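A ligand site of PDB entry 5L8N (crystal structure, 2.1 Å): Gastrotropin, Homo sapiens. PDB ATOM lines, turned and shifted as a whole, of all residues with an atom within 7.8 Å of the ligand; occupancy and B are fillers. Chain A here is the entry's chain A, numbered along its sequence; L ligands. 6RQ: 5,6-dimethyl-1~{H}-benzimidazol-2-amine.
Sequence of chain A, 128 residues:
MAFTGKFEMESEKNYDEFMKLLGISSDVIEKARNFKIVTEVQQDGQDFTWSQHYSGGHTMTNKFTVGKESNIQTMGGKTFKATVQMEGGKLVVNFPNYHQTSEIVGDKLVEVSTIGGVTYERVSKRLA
The side-chain carboxylate (OE2) of Glu 12 sits at hydrogen-bond distance from a nitrogen (N12) of the ligand.
O of Arg 33 is in hydrogen-bond range of N12 of the ligand (3.0 Å).
A nitrogen (N10) of the ligand lies close to the backbone carbonyl oxygen (O) of Ala 32 (2.8 Å).
N of Met 9 is in hydrogen-bond range of O of Ile 37 (2.9 Å).
The side-chain hydroxyl (OH) of Tyr 15 lies within hydrogen-bond range of the backbone NH (N) of Arg 33 (3.2 Å).
OE1 of Glu 12 sits at hydrogen-bond distance from OH of Tyr 120 (2.7 Å).
OH of Tyr 15 is in hydrogen-bond range of O of Ile 29.
OH of Tyr 120 is in hydrogen-bond range of NE of Arg 122.
Met 9 touches the ligand.
CE1 of Tyr 15 touches N9 of the ligand, 3.3 Å away.
CB of Phe 35 touches N10 of the ligand, at 3.95 Å.
Ile 37 touches the ligand.
CB of Met 75 touches C1 of the ligand, 3.5 Å away.
NH2 of Arg 122 touches C6 of the ligand, 3.6 Å away.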
ATOM      1  N   MET A   9      -5.946  21.551   3.133  1.00  0.00           N
ATOM      2  CA  MET A   9      -5.195  21.591   4.399  1.00  0.00           C
ATOM      3  C   MET A   9      -3.734  21.218   4.198  1.00  0.00           C
ATOM      4  O   MET A   9      -3.437  20.159   3.641  1.00  0.00           O
ATOM      5  CB  MET A   9      -5.820  20.656   5.449  1.00  0.00           C
ATOM      6  CG  MET A   9      -5.109  20.648   6.800  1.00  0.00           C
ATOM      7  SD  MET A   9      -5.949  19.620   8.026  1.00  0.00           S
ATOM      8  CE  MET A   9      -5.790  17.986   7.297  1.00  0.00           C
ATOM      9  N   GLU A  12      -1.159  22.152  10.414  1.00  0.00           N
ATOM     10  CA  GLU A  12      -2.022  22.272  11.584  1.00  0.00           C
ATOM     11  C   GLU A  12      -1.241  22.185  12.893  1.00  0.00           C
ATOM     12  O   GLU A  12      -0.290  21.410  12.989  1.00  0.00           O
ATOM     13  CB  GLU A  12      -3.182  21.259  11.546  1.00  0.00           C
ATOM     14  CG  GLU A  12      -2.758  19.805  11.573  1.00  0.00           C
ATOM     15  CD  GLU A  12      -3.890  18.840  11.286  1.00  0.00           C
ATOM     16  OE1 GLU A  12      -5.085  19.225  11.380  1.00  0.00           O
ATOM     17  OE2 GLU A  12      -3.575  17.680  10.958  1.00  0.00           O
ATOM     18  N   TYR A  15      -3.138  19.241  16.837  1.00  0.00           N
ATOM     19  CA  TYR A  15      -4.182  18.286  16.443  1.00  0.00           C
ATOM     20  C   TYR A  15      -4.441  17.247  17.550  1.00  0.00           C
ATOM     21  O   TYR A  15      -5.590  17.061  17.957  1.00  0.00           O
ATOM     22  CB  TYR A  15      -3.794  17.605  15.127  1.00  0.00           C
ATOM     23  CG  TYR A  15      -4.590  16.367  14.773  1.00  0.00           C
ATOM     24  CD1 TYR A  15      -5.875  16.455  14.240  1.00  0.00           C
ATOM     25  CD2 TYR A  15      -4.039  15.093  14.958  1.00  0.00           C
ATOM     26  CE1 TYR A  15      -6.598  15.319  13.904  1.00  0.00           C
ATOM     27  CE2 TYR A  15      -4.757  13.949  14.625  1.00  0.00           C
ATOM     28  CZ  TYR A  15      -6.027  14.063  14.106  1.00  0.00           C
ATOM     29  OH  TYR A  15      -6.740  12.925  13.784  1.00  0.00           O
ATOM     30  N   PHE A  18      -5.969  18.662  20.852  1.00  0.00           N
ATOM     31  CA  PHE A  18      -7.349  19.090  20.608  1.00  0.00           C
ATOM     32  C   PHE A  18      -8.317  17.918  20.494  1.00  0.00           C
ATOM     33  O   PHE A  18      -9.397  17.960  21.089  1.00  0.00           O
ATOM     34  CB  PHE A  18      -7.428  19.959  19.338  1.00  0.00           C
ATOM     35  CG  PHE A  18      -8.706  20.723  19.208  1.00  0.00           C
ATOM     36  CD1 PHE A  18      -8.943  21.855  19.983  1.00  0.00           C
ATOM     37  CD2 PHE A  18      -9.691  20.331  18.304  1.00  0.00           C
ATOM     38  CE1 PHE A  18     -10.126  22.572  19.861  1.00  0.00           C
ATOM     39  CE2 PHE A  18     -10.876  21.034  18.182  1.00  0.00           C
ATOM     40  CZ  PHE A  18     -11.089  22.168  18.956  1.00  0.00           C
ATOM     41  N   MET A  19      -7.925  16.894  19.745  1.00  0.00           N
ATOM     42  CA  MET A  19      -8.760  15.695  19.555  1.00  0.00           C
ATOM     43  C   MET A  19      -8.874  14.870  20.846  1.00  0.00           C
ATOM     44  O   MET A  19      -9.925  14.252  21.093  1.00  0.00           O
ATOM     45  CB  MET A  19      -8.215  14.809  18.432  1.00  0.00           C
ATOM     46  CG  MET A  19      -8.228  15.440  17.058  1.00  0.00           C
ATOM     47  SD  MET A  19      -9.889  15.604  16.360  1.00  0.00           S
ATOM     48  CE  MET A  19     -10.038  14.109  15.378  1.00  0.00           C
ATOM     49  N   LEU A  22     -11.384  16.657  22.975  1.00  0.00           N
ATOM     50  CA  LEU A  22     -12.731  16.262  22.516  1.00  0.00           C
ATOM     51  C   LEU A  22     -13.149  14.867  22.988  1.00  0.00           C
ATOM     52  O   LEU A  22     -14.351  14.562  23.055  1.00  0.00           O
ATOM     53  CB  LEU A  22     -12.832  16.353  20.975  1.00  0.00           C
ATOM     54  CG  LEU A  22     -12.805  17.761  20.370  1.00  0.00           C
ATOM     55  CD1 LEU A  22     -12.762  17.682  18.854  1.00  0.00           C
ATOM     56  CD2 LEU A  22     -13.994  18.598  20.822  1.00  0.00           C
ATOM     57  N   ILE A  24     -11.888  11.698  21.719  1.00  0.00           N
ATOM     58  CA  ILE A  24     -11.836  10.605  20.744  1.00  0.00           C
ATOM     59  C   ILE A  24     -10.621   9.719  21.043  1.00  0.00           C
ATOM     60  O   ILE A  24      -9.633  10.198  21.598  1.00  0.00           O
ATOM     61  CB  ILE A  24     -11.915  11.103  19.282  1.00  0.00           C
ATOM     62  CG1 ILE A  24     -10.629  11.773  18.808  1.00  0.00           C
ATOM     63  CG2 ILE A  24     -13.091  12.063  19.098  1.00  0.00           C
ATOM     64  CD1 ILE A  24     -10.292  11.410  17.392  1.00  0.00           C
ATOM     65  N   VAL A  28      -8.370   6.272  16.796  1.00  0.00           N
ATOM     66  CA  VAL A  28      -9.082   7.108  15.841  1.00  0.00           C
ATOM     67  C   VAL A  28      -8.269   8.381  15.546  1.00  0.00           C
ATOM     68  O   VAL A  28      -8.222   8.833  14.413  1.00  0.00           O
ATOM     69  CB  VAL A  28     -10.518   7.459  16.310  1.00  0.00           C
ATOM     70  CG1 VAL A  28     -11.203   8.434  15.353  1.00  0.00           C
ATOM     71  CG2 VAL A  28     -11.362   6.196  16.432  1.00  0.00           C
ATOM     72  N   ILE A  29      -7.625   8.941  16.578  1.00  0.00           N
ATOM     73  CA  ILE A  29      -6.716  10.076  16.384  1.00  0.00           C
ATOM     74  C   ILE A  29      -5.583   9.700  15.411  1.00  0.00           C
ATOM     75  O   ILE A  29      -5.261  10.465  14.511  1.00  0.00           O
ATOM     76  CB  ILE A  29      -6.104  10.590  17.717  1.00  0.00           C
ATOM     77  CG1 ILE A  29      -7.190  11.221  18.589  1.00  0.00           C
ATOM     78  CG2 ILE A  29      -5.013  11.632  17.449  1.00  0.00           C
ATOM     79  CD1 ILE A  29      -6.766  11.521  20.011  1.00  0.00           C
ATOM     80  N   GLU A  30      -5.003   8.508  15.600  1.00  0.00           N
ATOM     81  CA  GLU A  30      -3.900   8.025  14.775  1.00  0.00           C
ATOM     82  C   GLU A  30      -4.341   7.758  13.333  1.00  0.00           C
ATOM     83  O   GLU A  30      -3.671   8.189  12.387  1.00  0.00           O
ATOM     84  CB  GLU A  30      -3.292   6.763  15.376  1.00  0.00           C
ATOM     85  N   LYS A  31      -5.467   7.060  13.174  1.00  0.00           N
ATOM     86  CA  LYS A  31      -6.003   6.733  11.852  1.00  0.00           C
ATOM     87  C   LYS A  31      -6.467   7.987  11.091  1.00  0.00           C
ATOM     88  O   LYS A  31      -6.141   8.148   9.913  1.00  0.00           O
ATOM     89  CB  LYS A  31      -7.164   5.731  11.963  1.00  0.00           C
ATOM     90  N   ALA A  32      -7.205   8.866  11.769  1.00  0.00           N
ATOM     91  CA  ALA A  32      -7.720  10.096  11.151  1.00  0.00           C
ATOM     92  C   ALA A  32      -6.643  11.131  10.814  1.00  0.00           C
ATOM     93  O   ALA A  32      -6.848  11.966   9.918  1.00  0.00           O
ATOM     94  CB  ALA A  32      -8.790  10.731  12.039  1.00  0.00           C
ATOM     95  N   ARG A  33      -5.510  11.082  11.501  1.00  0.00           N
ATOM     96  CA  ARG A  33      -4.371  11.985  11.241  1.00  0.00           C
ATOM     97  C   ARG A  33      -4.018  12.149   9.753  1.00  0.00           C
ATOM     98  O   ARG A  33      -3.693  13.253   9.326  1.00  0.00           O
ATOM     99  CB  ARG A  33      -3.129  11.513  12.005  1.00  0.00           C
ATOM    100  CG  ARG A  33      -1.972  12.512  12.042  1.00  0.00           C
ATOM    101  CD  ARG A  33      -0.693  11.840  12.495  1.00  0.00           C
ATOM    102  NE  ARG A  33      -0.816  11.313  13.854  1.00  0.00           N
ATOM    103  CZ  ARG A  33      -0.773  12.045  14.970  1.00  0.00           C
ATOM    104  NH1 ARG A  33      -0.905  11.452  16.139  1.00  0.00           N
ATOM    105  NH2 ARG A  33      -0.589  13.377  14.921  1.00  0.00           N
ATOM    106  N   ASN A  34      -4.114  11.067   8.990  1.00  0.00           N
ATOM    107  CA  ASN A  34      -3.667  11.035   7.585  1.00  0.00           C
ATOM    108  C   ASN A  34      -4.708  11.558   6.581  1.00  0.00           C
ATOM    109  O   ASN A  34      -4.403  11.680   5.399  1.00  0.00           O
ATOM    110  CB  ASN A  34      -3.260   9.605   7.187  1.00  0.00           C
ATOM    111  CG  ASN A  34      -2.761   8.777   8.362  1.00  0.00           C
ATOM    112  OD1 ASN A  34      -1.776   9.129   9.023  1.00  0.00           O
ATOM    113  ND2 ASN A  34      -3.461   7.684   8.650  1.00  0.00           N
ATOM    114  N   PHE A  35      -5.932  11.848   7.047  1.00  0.00           N
ATOM    115  CA  PHE A  35      -7.007  12.373   6.190  1.00  0.00           C
ATOM    116  C   PHE A  35      -6.628  13.678   5.519  1.00  0.00           C
ATOM    117  O   PHE A  35      -6.082  14.580   6.164  1.00  0.00           O
ATOM    118  CB  PHE A  35      -8.295  12.609   7.001  1.00  0.00           C
ATOM    119  CG  PHE A  35      -9.112  11.365   7.281  1.00  0.00           C
ATOM    120  CD1 PHE A  35      -8.568  10.081   7.219  1.00  0.00           C
ATOM    121  CD2 PHE A  35     -10.455  11.496   7.642  1.00  0.00           C
ATOM    122  CE1 PHE A  35      -9.353   8.953   7.490  1.00  0.00           C
ATOM    123  CE2 PHE A  35     -11.240  10.382   7.923  1.00  0.00           C
ATOM    124  CZ  PHE A  35     -10.687   9.111   7.842  1.00  0.00           C
ATOM    125  N   LYS A  36      -6.907  13.771   4.223  1.00  0.00           N
ATOM    126  CA  LYS A  36      -6.858  15.029   3.489  1.00  0.00           C
ATOM    127  C   LYS A  36      -8.170  15.763   3.713  1.00  0.00           C
ATOM    128  O   LYS A  36      -9.236  15.130   3.752  1.00  0.00           O
ATOM    129  CB  LYS A  36      -6.642  14.773   1.999  1.00  0.00           C
ATOM    130  N   ILE A  37      -8.108  17.086   3.876  1.00  0.00           N
ATOM    131  CA  ILE A  37      -9.292  17.917   4.074  1.00  0.00           C
ATOM    132  C   ILE A  37      -9.294  19.058   3.076  1.00  0.00           C
ATOM    133  O   ILE A  37      -8.374  19.892   3.073  1.00  0.00           O
ATOM    134  CB  ILE A  37      -9.396  18.496   5.503  1.00  0.00           C
ATOM    135  CG1 ILE A  37      -9.495  17.361   6.528  1.00  0.00           C
ATOM    136  CG2 ILE A  37     -10.608  19.425   5.640  1.00  0.00           C
ATOM    137  CD1 ILE A  37      -9.443  17.810   7.972  1.00  0.00           C
ATOM    138  N   GLN A  52     -16.730  20.935   3.893  1.00  0.00           N
ATOM    139  CA  GLN A  52     -15.506  20.207   4.203  1.00  0.00           C
ATOM    140  C   GLN A  52     -15.578  18.834   3.559  1.00  0.00           C
ATOM    141  O   GLN A  52     -16.531  18.090   3.831  1.00  0.00           O
ATOM    142  CB  GLN A  52     -15.339  20.074   5.708  1.00  0.00           C
ATOM    143  CG  GLN A  52     -15.154  21.405   6.418  1.00  0.00           C
ATOM    144  CD  GLN A  52     -15.182  21.309   7.933  1.00  0.00           C
ATOM    145  OE1 GLN A  52     -15.837  20.436   8.507  1.00  0.00           O
ATOM    146  NE2 GLN A  52     -14.474  22.210   8.595  1.00  0.00           N
ATOM    147  N   TYR A  54     -13.662  15.291   3.152  1.00  0.00           N
ATOM    148  CA  TYR A  54     -12.661  14.423   3.777  1.00  0.00           C
ATOM    149  C   TYR A  54     -12.249  13.298   2.829  1.00  0.00           C
ATOM    150  O   TYR A  54     -12.970  12.985   1.877  1.00  0.00           O
ATOM    151  CB  TYR A  54     -13.198  13.836   5.085  1.00  0.00           C
ATOM    152  CG  TYR A  54     -13.746  14.886   6.031  1.00  0.00           C
ATOM    153  CD1 TYR A  54     -12.899  15.556   6.924  1.00  0.00           C
ATOM    154  CD2 TYR A  54     -15.102  15.235   6.027  1.00  0.00           C
ATOM    155  CE1 TYR A  54     -13.392  16.529   7.791  1.00  0.00           C
ATOM    156  CE2 TYR A  54     -15.599  16.201   6.882  1.00  0.00           C
ATOM    157  CZ  TYR A  54     -14.746  16.848   7.769  1.00  0.00           C
ATOM    158  OH  TYR A  54     -15.251  17.809   8.621  1.00  0.00           O
ATOM    159  N   SER A  55     -11.092  12.697   3.093  1.00  0.00           N
ATOM    160  CA  SER A  55     -10.591  11.558   2.308  1.00  0.00           C
ATOM    161  C   SER A  55     -11.567  10.384   2.395  1.00  0.00           C
ATOM    162  O   SER A  55     -12.012  10.035   3.492  1.00  0.00           O
ATOM    163  CB  SER A  55      -9.221  11.108   2.807  1.00  0.00           C
ATOM    164  OG  SER A  55      -8.240  12.092   2.578  1.00  0.00           O
ATOM    165  N   THR A  74     -20.203  19.025  12.566  1.00  0.00           N
ATOM    166  CA  THR A  74     -18.800  18.607  12.455  1.00  0.00           C
ATOM    167  C   THR A  74     -18.642  17.380  11.541  1.00  0.00           C
ATOM    168  O   THR A  74     -19.626  16.871  11.000  1.00  0.00           O
ATOM    169  CB  THR A  74     -18.215  18.300  13.850  1.00  0.00           C
ATOM    170  OG1 THR A  74     -18.913  17.175  14.420  1.00  0.00           O
ATOM    171  CG2 THR A  74     -18.362  19.510  14.769  1.00  0.00           C
ATOM    172  N   MET A  75     -17.393  16.932  11.375  1.00  0.00           N
ATOM    173  CA  MET A  75     -17.071  15.713  10.617  1.00  0.00           C
ATOM    174  C   MET A  75     -17.827  14.490  11.110  1.00  0.00           C
ATOM    175  O   MET A  75     -18.525  13.830  10.335  1.00  0.00           O
ATOM    176  CB  MET A  75     -15.566  15.409  10.694  1.00  0.00           C
ATOM    177  N   GLY A  76     -17.681  14.199  12.397  1.00  0.00           N
ATOM    178  CA  GLY A  76     -18.303  13.033  13.030  1.00  0.00           C
ATOM    179  C   GLY A  76     -19.828  13.055  13.110  1.00  0.00           C
ATOM    180  O   GLY A  76     -20.454  12.001  13.144  1.00  0.00           O
ATOM    181  N   TYR A 120      -6.083  24.975  18.642  1.00  0.00           N
ATOM    182  CA  TYR A 120      -5.853  24.239  17.391  1.00  0.00           C
ATOM    183  C   TYR A 120      -5.886  25.217  16.214  1.00  0.00           C
ATOM    184  O   TYR A 120      -6.818  26.002  16.113  1.00  0.00           O
ATOM    185  CB  TYR A 120      -6.916  23.149  17.225  1.00  0.00           C
ATOM    186  CG  TYR A 120      -6.995  22.504  15.842  1.00  0.00           C
ATOM    187  CD1 TYR A 120      -6.142  21.452  15.499  1.00  0.00           C
ATOM    188  CD2 TYR A 120      -7.934  22.930  14.905  1.00  0.00           C
ATOM    189  CE1 TYR A 120      -6.220  20.860  14.240  1.00  0.00           C
ATOM    190  CE2 TYR A 120      -8.013  22.338  13.645  1.00  0.00           C
ATOM    191  CZ  TYR A 120      -7.163  21.301  13.321  1.00  0.00           C
ATOM    192  OH  TYR A 120      -7.242  20.724  12.071  1.00  0.00           O
ATOM    193  N   ARG A 122      -5.545  25.395  11.856  1.00  0.00           N
ATOM    194  CA  ARG A 122      -5.470  24.716  10.554  1.00  0.00           C
ATOM    195  C   ARG A 122      -5.180  25.779   9.498  1.00  0.00           C
ATOM    196  O   ARG A 122      -5.858  26.805   9.448  1.00  0.00           O
ATOM    197  CB  ARG A 122      -6.794  24.010  10.269  1.00  0.00           C
ATOM    198  CG  ARG A 122      -6.817  23.192   8.997  1.00  0.00           C
ATOM    199  CD  ARG A 122      -8.229  22.719   8.691  1.00  0.00           C
ATOM    200  NE  ARG A 122      -8.699  21.739   9.674  1.00  0.00           N
ATOM    201  CZ  ARG A 122      -9.971  21.377   9.859  1.00  0.00           C
ATOM    202  NH1 ARG A 122     -10.957  21.917   9.140  1.00  0.00           N
ATOM    203  NH2 ARG A 122     -10.259  20.470  10.784  1.00  0.00           N
HETATM  204  C4  6RQ L   1      -8.546  15.078  10.614  1.00  0.00           C
HETATM  205  C5  6RQ L   1      -8.493  16.373  11.129  1.00  0.00           C
HETATM  206  C6  6RQ L   1      -9.623  17.019  11.599  1.00  0.00           C
HETATM  207  C7  6RQ L   1     -10.835  16.340  11.556  1.00  0.00           C
HETATM  208  C8  6RQ L   1     -12.081  17.023  12.065  1.00  0.00           C
HETATM  209  C11 6RQ L   1      -6.473  15.699  10.486  1.00  0.00           C
HETATM  210  C2  6RQ L   1     -10.907  15.020  11.036  1.00  0.00           C
HETATM  211  C1  6RQ L   1     -12.217  14.287  10.983  1.00  0.00           C
HETATM  212  C3  6RQ L   1      -9.760  14.391  10.550  1.00  0.00           C
HETATM  213  N9  6RQ L   1      -7.160  16.738  11.030  1.00  0.00           N
HETATM  214  N10 6RQ L   1      -7.278  14.687  10.205  1.00  0.00           N
HETATM  215  N12 6RQ L   1      -5.071  15.732  10.249  1.00  0.00           N
